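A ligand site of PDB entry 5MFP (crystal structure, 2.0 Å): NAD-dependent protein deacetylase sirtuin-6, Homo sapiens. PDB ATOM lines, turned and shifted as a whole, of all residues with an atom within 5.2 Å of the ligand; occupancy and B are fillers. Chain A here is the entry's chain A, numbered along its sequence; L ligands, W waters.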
ATOM      1  N   GLU A  16     -30.020   6.270 -30.124  1.00  0.00           N
ATOM      2  CA  GLU A  16     -31.119   5.289 -30.277  1.00  0.00           C
ATOM      3  C   GLU A  16     -31.880   5.542 -31.541  1.00  0.00           C
ATOM      4  O   GLU A  16     -31.921   6.652 -31.963  1.00  0.00           O
ATOM      5  CB  GLU A  16     -32.083   5.390 -29.095  1.00  0.00           C
ATOM      6  CG  GLU A  16     -31.392   5.101 -27.782  1.00  0.00           C
ATOM      7  CD  GLU A  16     -32.307   5.023 -26.628  1.00  0.00           C
ATOM      8  OE1 GLU A  16     -33.108   5.926 -26.517  1.00  0.00           O
ATOM      9  OE2 GLU A  16     -32.200   4.082 -25.813  1.00  0.00           O
ATOM     10  N   GLY A  46     -29.042  -9.852 -24.421  1.00  0.00           N
ATOM     11  CA  GLY A  46     -28.229  -9.049 -23.585  1.00  0.00           C
ATOM     12  C   GLY A  46     -28.951  -8.096 -22.707  1.00  0.00           C
ATOM     13  O   GLY A  46     -30.166  -8.238 -22.467  1.00  0.00           O
ATOM     14  N   ALA A  47     -28.165  -7.126 -22.184  1.00  0.00           N
ATOM     15  CA  ALA A  47     -28.549  -6.328 -21.039  1.00  0.00           C
ATOM     16  C   ALA A  47     -29.762  -5.473 -21.242  1.00  0.00           C
ATOM     17  O   ALA A  47     -30.545  -5.171 -20.293  1.00  0.00           O
ATOM     18  CB  ALA A  47     -27.391  -5.488 -20.558  1.00  0.00           C
ATOM     19  N   GLY A  48     -30.029  -5.246 -22.504  1.00  0.00           N
ATOM     20  CA  GLY A  48     -31.199  -4.492 -22.957  1.00  0.00           C
ATOM     21  C   GLY A  48     -32.545  -5.173 -22.560  1.00  0.00           C
ATOM     22  O   GLY A  48     -33.561  -4.483 -22.379  1.00  0.00           O
ATOM     23  N   THR A  51     -33.473  -3.819 -18.773  1.00  0.00           N
ATOM     24  CA  THR A  51     -33.631  -2.415 -18.464  1.00  0.00           C
ATOM     25  C   THR A  51     -35.032  -2.019 -17.983  1.00  0.00           C
ATOM     26  O   THR A  51     -35.164  -1.118 -17.123  1.00  0.00           O
ATOM     27  CB  THR A  51     -33.223  -1.549 -19.642  1.00  0.00           C
ATOM     28  OG1 THR A  51     -33.976  -1.842 -20.870  1.00  0.00           O
ATOM     29  CG2 THR A  51     -31.716  -1.601 -19.896  1.00  0.00           C
ATOM     30  N   ALA A  52     -36.049  -2.662 -18.532  1.00  0.00           N
ATOM     31  CA  ALA A  52     -37.454  -2.442 -18.074  1.00  0.00           C
ATOM     32  C   ALA A  52     -37.815  -3.025 -16.759  1.00  0.00           C
ATOM     33  O   ALA A  52     -38.934  -2.784 -16.271  1.00  0.00           O
ATOM     34  CB  ALA A  52     -38.403  -2.926 -19.116  1.00  0.00           C
ATOM     35  N   ASP A  57     -28.288  -1.099 -18.604  1.00  0.00           N
ATOM     36  CA  ASP A  57     -27.498  -1.902 -19.549  1.00  0.00           C
ATOM     37  C   ASP A  57     -26.030  -1.397 -19.392  1.00  0.00           C
ATOM     38  O   ASP A  57     -25.742  -0.617 -18.438  1.00  0.00           O
ATOM     39  CB  ASP A  57     -28.129  -1.919 -20.945  1.00  0.00           C
ATOM     40  CG  ASP A  57     -28.164  -0.489 -21.618  1.00  0.00           C
ATOM     41  OD1 ASP A  57     -27.479   0.428 -21.165  1.00  0.00           O
ATOM     42  OD2 ASP A  57     -28.926  -0.298 -22.531  1.00  0.00           O
ATOM     43  N   PHE A  58     -25.175  -1.748 -20.371  1.00  0.00           N
ATOM     44  CA  PHE A  58     -23.807  -1.338 -20.380  1.00  0.00           C
ATOM     45  C   PHE A  58     -23.489  -0.126 -21.254  1.00  0.00           C
ATOM     46  O   PHE A  58     -22.630   0.725 -20.887  1.00  0.00           O
ATOM     47  CB  PHE A  58     -22.856  -2.545 -20.698  1.00  0.00           C
ATOM     48  CG  PHE A  58     -22.854  -3.526 -19.602  1.00  0.00           C
ATOM     49  CD1 PHE A  58     -21.980  -3.423 -18.532  1.00  0.00           C
ATOM     50  CD2 PHE A  58     -23.788  -4.594 -19.642  1.00  0.00           C
ATOM     51  CE1 PHE A  58     -22.056  -4.351 -17.488  1.00  0.00           C
ATOM     52  CE2 PHE A  58     -23.833  -5.511 -18.616  1.00  0.00           C
ATOM     53  CZ  PHE A  58     -23.027  -5.333 -17.501  1.00  0.00           C
ATOM     54  N   ARG A  59     -24.100  -0.100 -22.460  1.00  0.00           N
ATOM     55  CA  ARG A  59     -23.672   0.749 -23.564  1.00  0.00           C
ATOM     56  C   ARG A  59     -24.741   1.601 -24.122  1.00  0.00           C
ATOM     57  O   ARG A  59     -24.490   2.402 -25.046  1.00  0.00           O
ATOM     58  CB  ARG A  59     -22.990  -0.052 -24.667  1.00  0.00           C
ATOM     59  CG  ARG A  59     -21.699  -0.687 -24.202  1.00  0.00           C
ATOM     60  CD  ARG A  59     -20.969  -1.502 -25.243  1.00  0.00           C
ATOM     61  NE  ARG A  59     -19.882  -2.290 -24.715  1.00  0.00           N
ATOM     62  CZ  ARG A  59     -20.009  -3.479 -24.093  1.00  0.00           C
ATOM     63  NH1 ARG A  59     -21.191  -4.101 -23.953  1.00  0.00           N
ATOM     64  NH2 ARG A  59     -18.944  -4.115 -23.665  1.00  0.00           N
ATOM     65  N   GLY A  60     -25.899   1.583 -23.449  1.00  0.00           N
ATOM     66  CA  GLY A  60     -27.042   2.435 -23.743  1.00  0.00           C
ATOM     67  C   GLY A  60     -26.761   3.890 -23.245  1.00  0.00           C
ATOM     68  O   GLY A  60     -25.700   4.189 -22.622  1.00  0.00           O
ATOM     69  N   TRP A  65     -21.094   1.521 -18.629  1.00  0.00           N
ATOM     70  CA  TRP A  65     -19.844   2.037 -19.252  1.00  0.00           C
ATOM     71  C   TRP A  65     -20.029   3.412 -19.880  1.00  0.00           C
ATOM     72  O   TRP A  65     -19.116   4.250 -19.853  1.00  0.00           O
ATOM     73  CB  TRP A  65     -19.314   1.105 -20.318  1.00  0.00           C
ATOM     74  CG  TRP A  65     -19.093  -0.345 -19.946  1.00  0.00           C
ATOM     75  CD1 TRP A  65     -19.226  -1.390 -20.817  1.00  0.00           C
ATOM     76  CD2 TRP A  65     -18.634  -0.904 -18.720  1.00  0.00           C
ATOM     77  NE1 TRP A  65     -18.906  -2.559 -20.199  1.00  0.00           N
ATOM     78  CE2 TRP A  65     -18.597  -2.308 -18.891  1.00  0.00           C
ATOM     79  CE3 TRP A  65     -18.314  -0.378 -17.450  1.00  0.00           C
ATOM     80  CZ2 TRP A  65     -18.180  -3.186 -17.903  1.00  0.00           C
ATOM     81  CZ3 TRP A  65     -17.967  -1.226 -16.454  1.00  0.00           C
ATOM     82  CH2 TRP A  65     -17.892  -2.653 -16.678  1.00  0.00           C
ATOM     83  N   GLN A 107     -25.802 -13.293 -22.512  1.00  0.00           N
ATOM     84  CA  GLN A 107     -24.704 -12.636 -21.915  1.00  0.00           C
ATOM     85  C   GLN A 107     -24.969 -12.012 -20.524  1.00  0.00           C
ATOM     86  O   GLN A 107     -24.039 -11.478 -19.907  1.00  0.00           O
ATOM     87  CB  GLN A 107     -24.279 -11.553 -22.887  1.00  0.00           C
ATOM     88  CG  GLN A 107     -23.737 -12.063 -24.181  1.00  0.00           C
ATOM     89  CD  GLN A 107     -23.510 -10.986 -25.212  1.00  0.00           C
ATOM     90  OE1 GLN A 107     -22.492 -10.276 -25.170  1.00  0.00           O
ATOM     91  NE2 GLN A 107     -24.451 -10.861 -26.176  1.00  0.00           N
ATOM     92  N   ASN A 108     -26.195 -12.079 -20.010  1.00  0.00           N
ATOM     93  CA  ASN A 108     -26.541 -11.400 -18.766  1.00  0.00           C
ATOM     94  C   ASN A 108     -26.129 -12.242 -17.564  1.00  0.00           C
ATOM     95  O   ASN A 108     -26.340 -13.465 -17.515  1.00  0.00           O
ATOM     96  CB  ASN A 108     -28.032 -11.164 -18.715  1.00  0.00           C
ATOM     97  CG  ASN A 108     -28.476 -10.314 -19.879  1.00  0.00           C
ATOM     98  OD1 ASN A 108     -27.640  -9.655 -20.455  1.00  0.00           O
ATOM     99  ND2 ASN A 108     -29.736 -10.327 -20.215  1.00  0.00           N
ATOM    100  N   HIS A 127     -21.538 -15.392 -19.616  1.00  0.00           N
ATOM    101  CA  HIS A 127     -20.709 -14.516 -18.768  1.00  0.00           C
ATOM    102  C   HIS A 127     -20.880 -14.781 -17.306  1.00  0.00           C
ATOM    103  O   HIS A 127     -20.264 -14.088 -16.500  1.00  0.00           O
ATOM    104  CB  HIS A 127     -20.991 -13.008 -19.109  1.00  0.00           C
ATOM    105  CG  HIS A 127     -20.726 -12.688 -20.552  1.00  0.00           C
ATOM    106  ND1 HIS A 127     -21.077 -11.500 -21.150  1.00  0.00           N
ATOM    107  CD2 HIS A 127     -20.066 -13.419 -21.508  1.00  0.00           C
ATOM    108  CE1 HIS A 127     -20.732 -11.540 -22.417  1.00  0.00           C
ATOM    109  NE2 HIS A 127     -20.064 -12.660 -22.641  1.00  0.00           N
ATOM    110  N   TRP A 182     -12.475  -9.642 -17.057  1.00  0.00           N
ATOM    111  CA  TRP A 182     -11.984  -9.348 -18.411  1.00  0.00           C
ATOM    112  C   TRP A 182     -11.041 -10.401 -18.981  1.00  0.00           C
ATOM    113  O   TRP A 182     -11.208 -10.783 -20.110  1.00  0.00           O
ATOM    114  CB  TRP A 182     -11.305  -7.954 -18.445  1.00  0.00           C
ATOM    115  CG  TRP A 182     -12.346  -6.853 -18.398  1.00  0.00           C
ATOM    116  CD1 TRP A 182     -12.644  -6.056 -17.317  1.00  0.00           C
ATOM    117  CD2 TRP A 182     -13.261  -6.473 -19.448  1.00  0.00           C
ATOM    118  NE1 TRP A 182     -13.675  -5.193 -17.645  1.00  0.00           N
ATOM    119  CE2 TRP A 182     -14.074  -5.434 -18.947  1.00  0.00           C
ATOM    120  CE3 TRP A 182     -13.464  -6.920 -20.785  1.00  0.00           C
ATOM    121  CZ2 TRP A 182     -15.086  -4.820 -19.725  1.00  0.00           C
ATOM    122  CZ3 TRP A 182     -14.476  -6.298 -21.553  1.00  0.00           C
ATOM    123  CH2 TRP A 182     -15.270  -5.260 -21.011  1.00  0.00           C
ATOM    124  N   GLY A 208     -31.815  -6.973 -27.323  1.00  0.00           N
ATOM    125  CA  GLY A 208     -31.141  -6.113 -26.342  1.00  0.00           C
ATOM    126  C   GLY A 208     -29.710  -6.429 -26.066  1.00  0.00           C
ATOM    127  O   GLY A 208     -29.247  -6.383 -24.882  1.00  0.00           O
ATOM    128  N   THR A 209     -29.000  -6.683 -27.166  1.00  0.00           N
ATOM    129  CA  THR A 209     -27.543  -6.790 -27.239  1.00  0.00           C
ATOM    130  C   THR A 209     -26.928  -5.991 -28.435  1.00  0.00           C
ATOM    131  O   THR A 209     -27.460  -6.024 -29.547  1.00  0.00           O
ATOM    132  CB  THR A 209     -26.984  -8.236 -27.230  1.00  0.00           C
ATOM    133  OG1 THR A 209     -25.536  -8.144 -27.293  1.00  0.00           O
ATOM    134  CG2 THR A 209     -27.498  -9.129 -28.299  1.00  0.00           C
ATOM    135  N   SER A 210     -25.870  -5.204 -28.137  1.00  0.00           N
ATOM    136  CA  SER A 210     -25.154  -4.456 -29.122  1.00  0.00           C
ATOM    137  C   SER A 210     -24.123  -5.341 -29.870  1.00  0.00           C
ATOM    138  O   SER A 210     -23.549  -4.883 -30.845  1.00  0.00           O
ATOM    139  CB  SER A 210     -24.493  -3.181 -28.554  1.00  0.00           C
ATOM    140  OG  SER A 210     -23.530  -3.410 -27.581  1.00  0.00           O
ATOM    141  N   LEU A 211     -23.950  -6.587 -29.426  1.00  0.00           N
ATOM    142  CA  LEU A 211     -23.131  -7.612 -30.150  1.00  0.00           C
ATOM    143  C   LEU A 211     -21.641  -7.291 -30.303  1.00  0.00           C
ATOM    144  O   LEU A 211     -20.934  -7.832 -31.210  1.00  0.00           O
ATOM    145  CB  LEU A 211     -23.725  -7.992 -31.513  1.00  0.00           C
ATOM    146  CG  LEU A 211     -25.206  -8.466 -31.545  1.00  0.00           C
ATOM    147  CD1 LEU A 211     -25.806  -8.553 -32.954  1.00  0.00           C
ATOM    148  CD2 LEU A 211     -25.271  -9.817 -30.842  1.00  0.00           C
ATOM    149  N   GLN A 212     -21.148  -6.464 -29.385  1.00  0.00           N
ATOM    150  CA  GLN A 212     -19.800  -5.946 -29.463  1.00  0.00           C
ATOM    151  C   GLN A 212     -18.740  -6.934 -28.869  1.00  0.00           C
ATOM    152  O   GLN A 212     -17.531  -6.702 -29.028  1.00  0.00           O
ATOM    153  CB  GLN A 212     -19.733  -4.592 -28.816  1.00  0.00           C
ATOM    154  CG  GLN A 212     -20.449  -3.525 -29.555  1.00  0.00           C
ATOM    155  CD  GLN A 212     -20.200  -2.163 -29.004  1.00  0.00           C
ATOM    156  OE1 GLN A 212     -19.073  -1.722 -28.992  1.00  0.00           O
ATOM    157  NE2 GLN A 212     -21.248  -1.439 -28.625  1.00  0.00           N
ATOM    158  N   ILE A 213     -19.162  -7.958 -28.121  1.00  0.00           N
ATOM    159  CA  ILE A 213     -18.246  -8.788 -27.351  1.00  0.00           C
ATOM    160  C   ILE A 213     -18.051 -10.065 -28.097  1.00  0.00           C
ATOM    161  O   ILE A 213     -19.020 -10.727 -28.428  1.00  0.00           O
ATOM    162  CB  ILE A 213     -18.828  -9.242 -25.989  1.00  0.00           C
ATOM    163  CG1 ILE A 213     -18.839  -8.111 -25.009  1.00  0.00           C
ATOM    164  CG2 ILE A 213     -17.996 -10.421 -25.421  1.00  0.00           C
ATOM    165  CD1 ILE A 213     -17.461  -7.569 -24.604  1.00  0.00           C
ATOM    166  N   VAL A 233     -32.998  -7.247 -32.737  1.00  0.00           N
ATOM    167  CA  VAL A 233     -33.993  -6.325 -32.136  1.00  0.00           C
ATOM    168  C   VAL A 233     -33.178  -5.551 -31.120  1.00  0.00           C
ATOM    169  O   VAL A 233     -32.568  -6.121 -30.223  1.00  0.00           O
ATOM    170  CB  VAL A 233     -35.151  -7.042 -31.442  1.00  0.00           C
ATOM    171  CG1 VAL A 233     -36.124  -6.046 -30.792  1.00  0.00           C
ATOM    172  CG2 VAL A 233     -35.945  -7.941 -32.439  1.00  0.00           C
ATOM    173  N   ASN A 234     -33.106  -4.222 -31.326  1.00  0.00           N
ATOM    174  CA  ASN A 234     -32.272  -3.368 -30.516  1.00  0.00           C
ATOM    175  C   ASN A 234     -32.591  -1.901 -30.764  1.00  0.00           C
ATOM    176  O   ASN A 234     -32.758  -1.473 -31.918  1.00  0.00           O
ATOM    177  CB  ASN A 234     -30.772  -3.576 -30.840  1.00  0.00           C
ATOM    178  CG  ASN A 234     -29.899  -3.333 -29.629  1.00  0.00           C
ATOM    179  OD1 ASN A 234     -30.090  -3.954 -28.580  1.00  0.00           O
ATOM    180  ND2 ASN A 234     -28.987  -2.381 -29.733  1.00  0.00           N
ATOM    181  N   LEU A 235     -32.571  -1.102 -29.704  1.00  0.00           N
ATOM    182  CA  LEU A 235     -32.658   0.342 -29.857  1.00  0.00           C
ATOM    183  C   LEU A 235     -31.461   1.144 -30.578  1.00  0.00           C
ATOM    184  O   LEU A 235     -31.702   2.009 -31.395  1.00  0.00           O
ATOM    185  CB  LEU A 235     -32.961   0.969 -28.517  1.00  0.00           C
ATOM    186  CG  LEU A 235     -34.396   0.758 -27.966  1.00  0.00           C
ATOM    187  CD1 LEU A 235     -34.476   1.196 -26.496  1.00  0.00           C
ATOM    188  CD2 LEU A 235     -35.424   1.485 -28.819  1.00  0.00           C
ATOM    189  N   GLN A 236     -30.241   0.770 -30.313  1.00  0.00           N
ATOM    190  CA  GLN A 236     -29.042   1.334 -30.897  1.00  0.00           C
ATOM    191  C   GLN A 236     -28.647   0.429 -32.076  1.00  0.00           C
ATOM    192  O   GLN A 236     -29.045  -0.752 -32.187  1.00  0.00           O
ATOM    193  CB  GLN A 236     -27.875   1.260 -29.904  1.00  0.00           C
ATOM    194  CG  GLN A 236     -27.943   2.290 -28.845  1.00  0.00           C
ATOM    195  CD  GLN A 236     -26.908   2.168 -27.756  1.00  0.00           C
ATOM    196  OE1 GLN A 236     -26.478   1.081 -27.370  1.00  0.00           O
ATOM    197  NE2 GLN A 236     -26.545   3.332 -27.184  1.00  0.00           N
ATOM    198  N   PRO A 237     -27.761   0.932 -32.929  1.00  0.00           N
ATOM    199  CA  PRO A 237     -26.991   0.102 -33.802  1.00  0.00           C
ATOM    200  C   PRO A 237     -26.260  -0.984 -33.027  1.00  0.00           C
ATOM    201  O   PRO A 237     -25.892  -0.809 -31.867  1.00  0.00           O
ATOM    202  CB  PRO A 237     -25.920   1.084 -34.443  1.00  0.00           C
ATOM    203  CG  PRO A 237     -26.309   2.464 -33.987  1.00  0.00           C
ATOM    204  CD  PRO A 237     -27.446   2.377 -33.022  1.00  0.00           C
ATOM    205  N   GLY A 250     -36.891  -0.799 -31.552  1.00  0.00           N
ATOM    206  CA  GLY A 250     -38.091  -0.609 -30.716  1.00  0.00           C
ATOM    207  C   GLY A 250     -37.797  -1.234 -29.370  1.00  0.00           C
ATOM    208  O   GLY A 250     -36.804  -1.981 -29.224  1.00  0.00           O
ATOM    209  N   TYR A 251     -38.599  -0.897 -28.377  1.00  0.00           N
ATOM    210  CA  TYR A 251     -38.494  -1.511 -27.048  1.00  0.00           C
ATOM    211  C   TYR A 251     -38.781  -3.015 -27.167  1.00  0.00           C
ATOM    212  O   TYR A 251     -39.765  -3.381 -27.804  1.00  0.00           O
ATOM    213  CB  TYR A 251     -39.467  -0.859 -26.059  1.00  0.00           C
ATOM    214  CG  TYR A 251     -39.066   0.577 -25.788  1.00  0.00           C
ATOM    215  CD1 TYR A 251     -37.993   0.866 -24.974  1.00  0.00           C
ATOM    216  CD2 TYR A 251     -39.761   1.640 -26.390  1.00  0.00           C
ATOM    217  CE1 TYR A 251     -37.648   2.165 -24.696  1.00  0.00           C
ATOM    218  CE2 TYR A 251     -39.408   2.943 -26.134  1.00  0.00           C
ATOM    219  CZ  TYR A 251     -38.316   3.181 -25.302  1.00  0.00           C
ATOM    220  OH  TYR A 251     -37.920   4.441 -25.054  1.00  0.00           O
ATOM    221  N   VAL A 252     -37.877  -3.887 -26.664  1.00  0.00           N
ATOM    222  CA  VAL A 252     -38.094  -5.273 -26.754  1.00  0.00           C
ATOM    223  C   VAL A 252     -39.426  -5.764 -26.166  1.00  0.00           C
ATOM    224  O   VAL A 252     -40.009  -6.632 -26.746  1.00  0.00           O
ATOM    225  CB  VAL A 252     -36.966  -6.179 -26.270  1.00  0.00           C
ATOM    226  CG1 VAL A 252     -35.825  -6.115 -27.243  1.00  0.00           C
ATOM    227  CG2 VAL A 252     -36.495  -5.832 -24.824  1.00  0.00           C
HETATM  228  N1  LIG L   1     -35.432  -2.549 -25.817  1.00  0.00           N
HETATM  229  C1  LIG L   1     -34.600  -2.690 -26.862  1.00  0.00           C
HETATM  230  N2  LIG L   1     -33.264  -2.447 -26.788  1.00  0.00           N
HETATM  231  C2  LIG L   1     -32.746  -2.056 -25.571  1.00  0.00           C
HETATM  232  C3  LIG L   1     -33.603  -1.774 -24.462  1.00  0.00           C
HETATM  233  C4  LIG L   1     -35.031  -2.099 -24.618  1.00  0.00           C
HETATM  234  N3  LIG L   1     -35.892  -1.968 -23.584  1.00  0.00           N
HETATM  235  N4  LIG L   1     -32.835  -1.369 -23.421  1.00  0.00           N
HETATM  236  C5  LIG L   1     -31.578  -1.298 -23.881  1.00  0.00           C
HETATM  237  N5  LIG L   1     -31.565  -1.665 -25.178  1.00  0.00           N
HETATM  238  P1  LIG L   1     -24.926  -3.518 -24.120  1.00  0.00           P
HETATM  239  P2  LIG L   1     -24.599  -6.403 -24.011  1.00  0.00           P
HETATM  240  C6  LIG L   1     -30.389  -1.796 -26.059  1.00  0.00           C
HETATM  241  O1  LIG L   1     -23.747  -3.436 -25.049  1.00  0.00           O
HETATM  242  O2  LIG L   1     -25.421  -7.366 -23.236  1.00  0.00           O
HETATM  243  C7  LIG L   1     -20.393  -6.028 -21.043  1.00  0.00           C
HETATM  244  O3  LIG L   1     -19.043  -5.733 -20.692  1.00  0.00           O
HETATM  245  C8  LIG L   1     -29.312  -0.702 -26.018  1.00  0.00           C
HETATM  246  O4  LIG L   1     -29.657   0.177 -27.043  1.00  0.00           O
HETATM  247  O5  LIG L   1     -25.244  -2.515 -23.092  1.00  0.00           O
HETATM  248  O6  LIG L   1     -24.596  -6.481 -25.475  1.00  0.00           O
HETATM  249  C9  LIG L   1     -20.956  -7.221 -20.196  1.00  0.00           C
HETATM  250  O7  LIG L   1     -19.903  -8.200 -19.953  1.00  0.00           O
HETATM  251  C10 LIG L   1     -27.983  -1.519 -26.190  1.00  0.00           C
HETATM  252  O8  LIG L   1     -27.560  -1.434 -27.481  1.00  0.00           O
HETATM  253  O9  LIG L   1     -25.013  -4.999 -23.415  1.00  0.00           O
HETATM  254  C11 LIG L   1     -22.081  -7.811 -21.121  1.00  0.00           C
HETATM  255  O10 LIG L   1     -22.444  -9.194 -20.743  1.00  0.00           O
HETATM  256  C12 LIG L   1     -28.391  -2.991 -25.875  1.00  0.00           C
HETATM  257  O11 LIG L   1     -29.793  -2.968 -25.590  1.00  0.00           O
HETATM  258  C13 LIG L   1     -21.349  -7.683 -22.441  1.00  0.00           C
HETATM  259  O12 LIG L   1     -20.560  -6.437 -22.414  1.00  0.00           O
HETATM  260  C14 LIG L   1     -27.555  -3.506 -24.781  1.00  0.00           C
HETATM  261  O13 LIG L   1     -26.149  -3.545 -25.147  1.00  0.00           O
HETATM  262  C15 LIG L   1     -22.276  -7.595 -23.600  1.00  0.00           C
HETATM  263  O14 LIG L   1     -23.095  -6.419 -23.403  1.00  0.00           O
HETATM  264  O   HOH W   1     -30.497   1.743 -22.901  1.00  0.00           O
HETATM  265  O   HOH W   2     -30.672   2.099 -25.696  1.00  0.00           O
HETATM  266  O   HOH W   3     -36.110  -4.139 -21.079  1.00  0.00           O
HETATM  267  O   HOH W   4     -20.362  -9.583 -17.768  1.00  0.00           O
HETATM  268  O   HOH W   5     -25.094  -8.544 -20.761  1.00  0.00           O
HETATM  269  O   HOH W   6     -33.297   1.175 -22.407  1.00  0.00           O
HETATM  270  O   HOH W   7     -23.601  -9.375 -17.903  1.00  0.00           O
HETATM  271  O   HOH W   8     -22.227  -5.838 -26.851  1.00  0.00           O
HETATM  272  O   HOH W   9     -38.394  -3.453 -23.205  1.00  0.00           O
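The backbone carbonyl oxygen of Gly 48 lies close to a nitrogen (N4) of the ligand.
CA of Gly 46 touches O2 of the ligand (3.3 Å).
Asp 57 touches the ligand (OD2 to C5, 3.1 Å).
Trp 182 touches the ligand (CH2 to O3, 3.8 Å).
O of Gly 208 touches C14 of the ligand, 3.3 Å away.
Ile 213 touches the ligand.
Gly 250 touches the ligand.
CA of Tyr 251 touches N1 of the ligand (3.5 Å).
Hydrophobic or aromatic side chains within 4 Å of the ligand: Ala 47, Phe 58, Trp 65, His 127, Trp 182, Ile 213, Leu 235, Tyr 251 and Val 252.
Of the 29 residues printed, 21 come within 4 Å of the ligand.
The nearest printed residue that does not touch the ligand is Leu 211 (4.005 Å).
An oxygen (O6) of the ligand sits at hydrogen-bond distance from the backbone NH (N) of Ser 210, at 3.2 Å.
An oxygen (O1) of the ligand sits at hydrogen-bond distance from the side-chain hydroxyl (OG) of Ser 210 (2.5 Å).
An oxygen (O6) of the ligand is in hydrogen-bond range of the side-chain hydroxyl of Thr 209 (2.6 Å).
O10 of the ligand is in hydrogen-bond range of ND1 of His 127.
The backbone NH (N) of Gln 236 sits close to an oxygen (O4) of the ligand (3.4 Å).
The side-chain amide oxygen of Gln 236 lies within hydrogen-bond range of an oxygen (O8) of the ligand, at 2.7 Å.
An oxygen (O5) of the ligand is in hydrogen-bond range of the backbone NH of Arg 59.
An oxygen (O1) of the ligand lies within salt-bridge range of the guanidinium group (NH1) of Arg 59 (2.9 Å).
The backbone NH (N) of Phe 58 sits at hydrogen-bond distance from an oxygen (O5) of the ligand, 2.8 Å away.
An oxygen (O8) of the ligand is in hydrogen-bond range of the side-chain amide nitrogen (ND2) of Asn 234, 2.8 Å away.
A nitrogen (N4) of the ligand lies within hydrogen-bond range of the side-chain hydroxyl (OG1) of Thr 51.
O of Gln 107 lies within hydrogen-bond range of O10 of the ligand (2.9 Å).
N of Val 252 lies within hydrogen-bond range of N1 of the ligand, at 2.9 Å.
The backbone NH (N) of Ala 47 lies within hydrogen-bond range of an oxygen (O2) of the ligand, at 2.9 Å.
An oxygen (O3) of the ligand lies within hydrogen-bond range of the indole nitrogen (NE1) of Trp 65, 3.2 Å away.
The backbone NH of Leu 235 lies within hydrogen-bond range of a nitrogen (N2) of the ligand (3.3 Å).
The side-chain amide nitrogen (NE2) of Gln 212 sits at hydrogen-bond distance from the side-chain hydroxyl (OG) of Ser 210, at 3.2 Å.
O of Gln 107 is in hydrogen-bond range of ND1 of His 127.
O of Arg 59 sits at hydrogen-bond distance from NE2 of Gln 236 (3.1 Å).
The side-chain hydroxyl (OG1) of Thr 51 is in hydrogen-bond range of the backbone carbonyl oxygen (O) of Gly 48, at 3.1 Å.
The backbone NH (N) of Ala 47 is in hydrogen-bond range of the backbone carbonyl oxygen (O) of Gly 208 (3.0 Å).
The backbone NH (N) of Ala 47 is in hydrogen-bond range of the side-chain amide oxygen (OD1) of Asn 108, 3.1 Å away.
The backbone carbonyl oxygen (O) of Gly 208 lies within hydrogen-bond range of the backbone NH (N) of Gly 48.
O of Val 233 is in hydrogen-bond range of N of Gly 208, 3.1 Å away.
Water W2 lies within hydrogen-bond range of OE2 of Glu 16 and O4 of the ligand.
Water W5 lies within hydrogen-bond range of an oxygen (O10) of the ligand (2.7 Å), the side-chain amide oxygen of Asn 108 (2.8 Å) and the backbone carbonyl oxygen of Gln 107 (3.2 Å).
Water W6 lies within hydrogen-bond range of a nitrogen (N4) of the ligand (2.8 Å) and the side-chain hydroxyl of Thr 51 (3.5 Å).
Water W8 lies within hydrogen-bond range of O6 of the ligand (2.8 Å), N of Gln 212 (2.8 Å), OG of Ser 210 (2.9 Å) and N of Leu 211 (3.2 Å).
Water W7 lies within hydrogen-bond range of O of Gln 107 (2.9 Å) and O10 of the ligand (3.1 Å).
Water W3 lies within hydrogen-bond range of O of Gly 48, N of Ala 52, OG1 of Thr 51 and N3 of the ligand.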
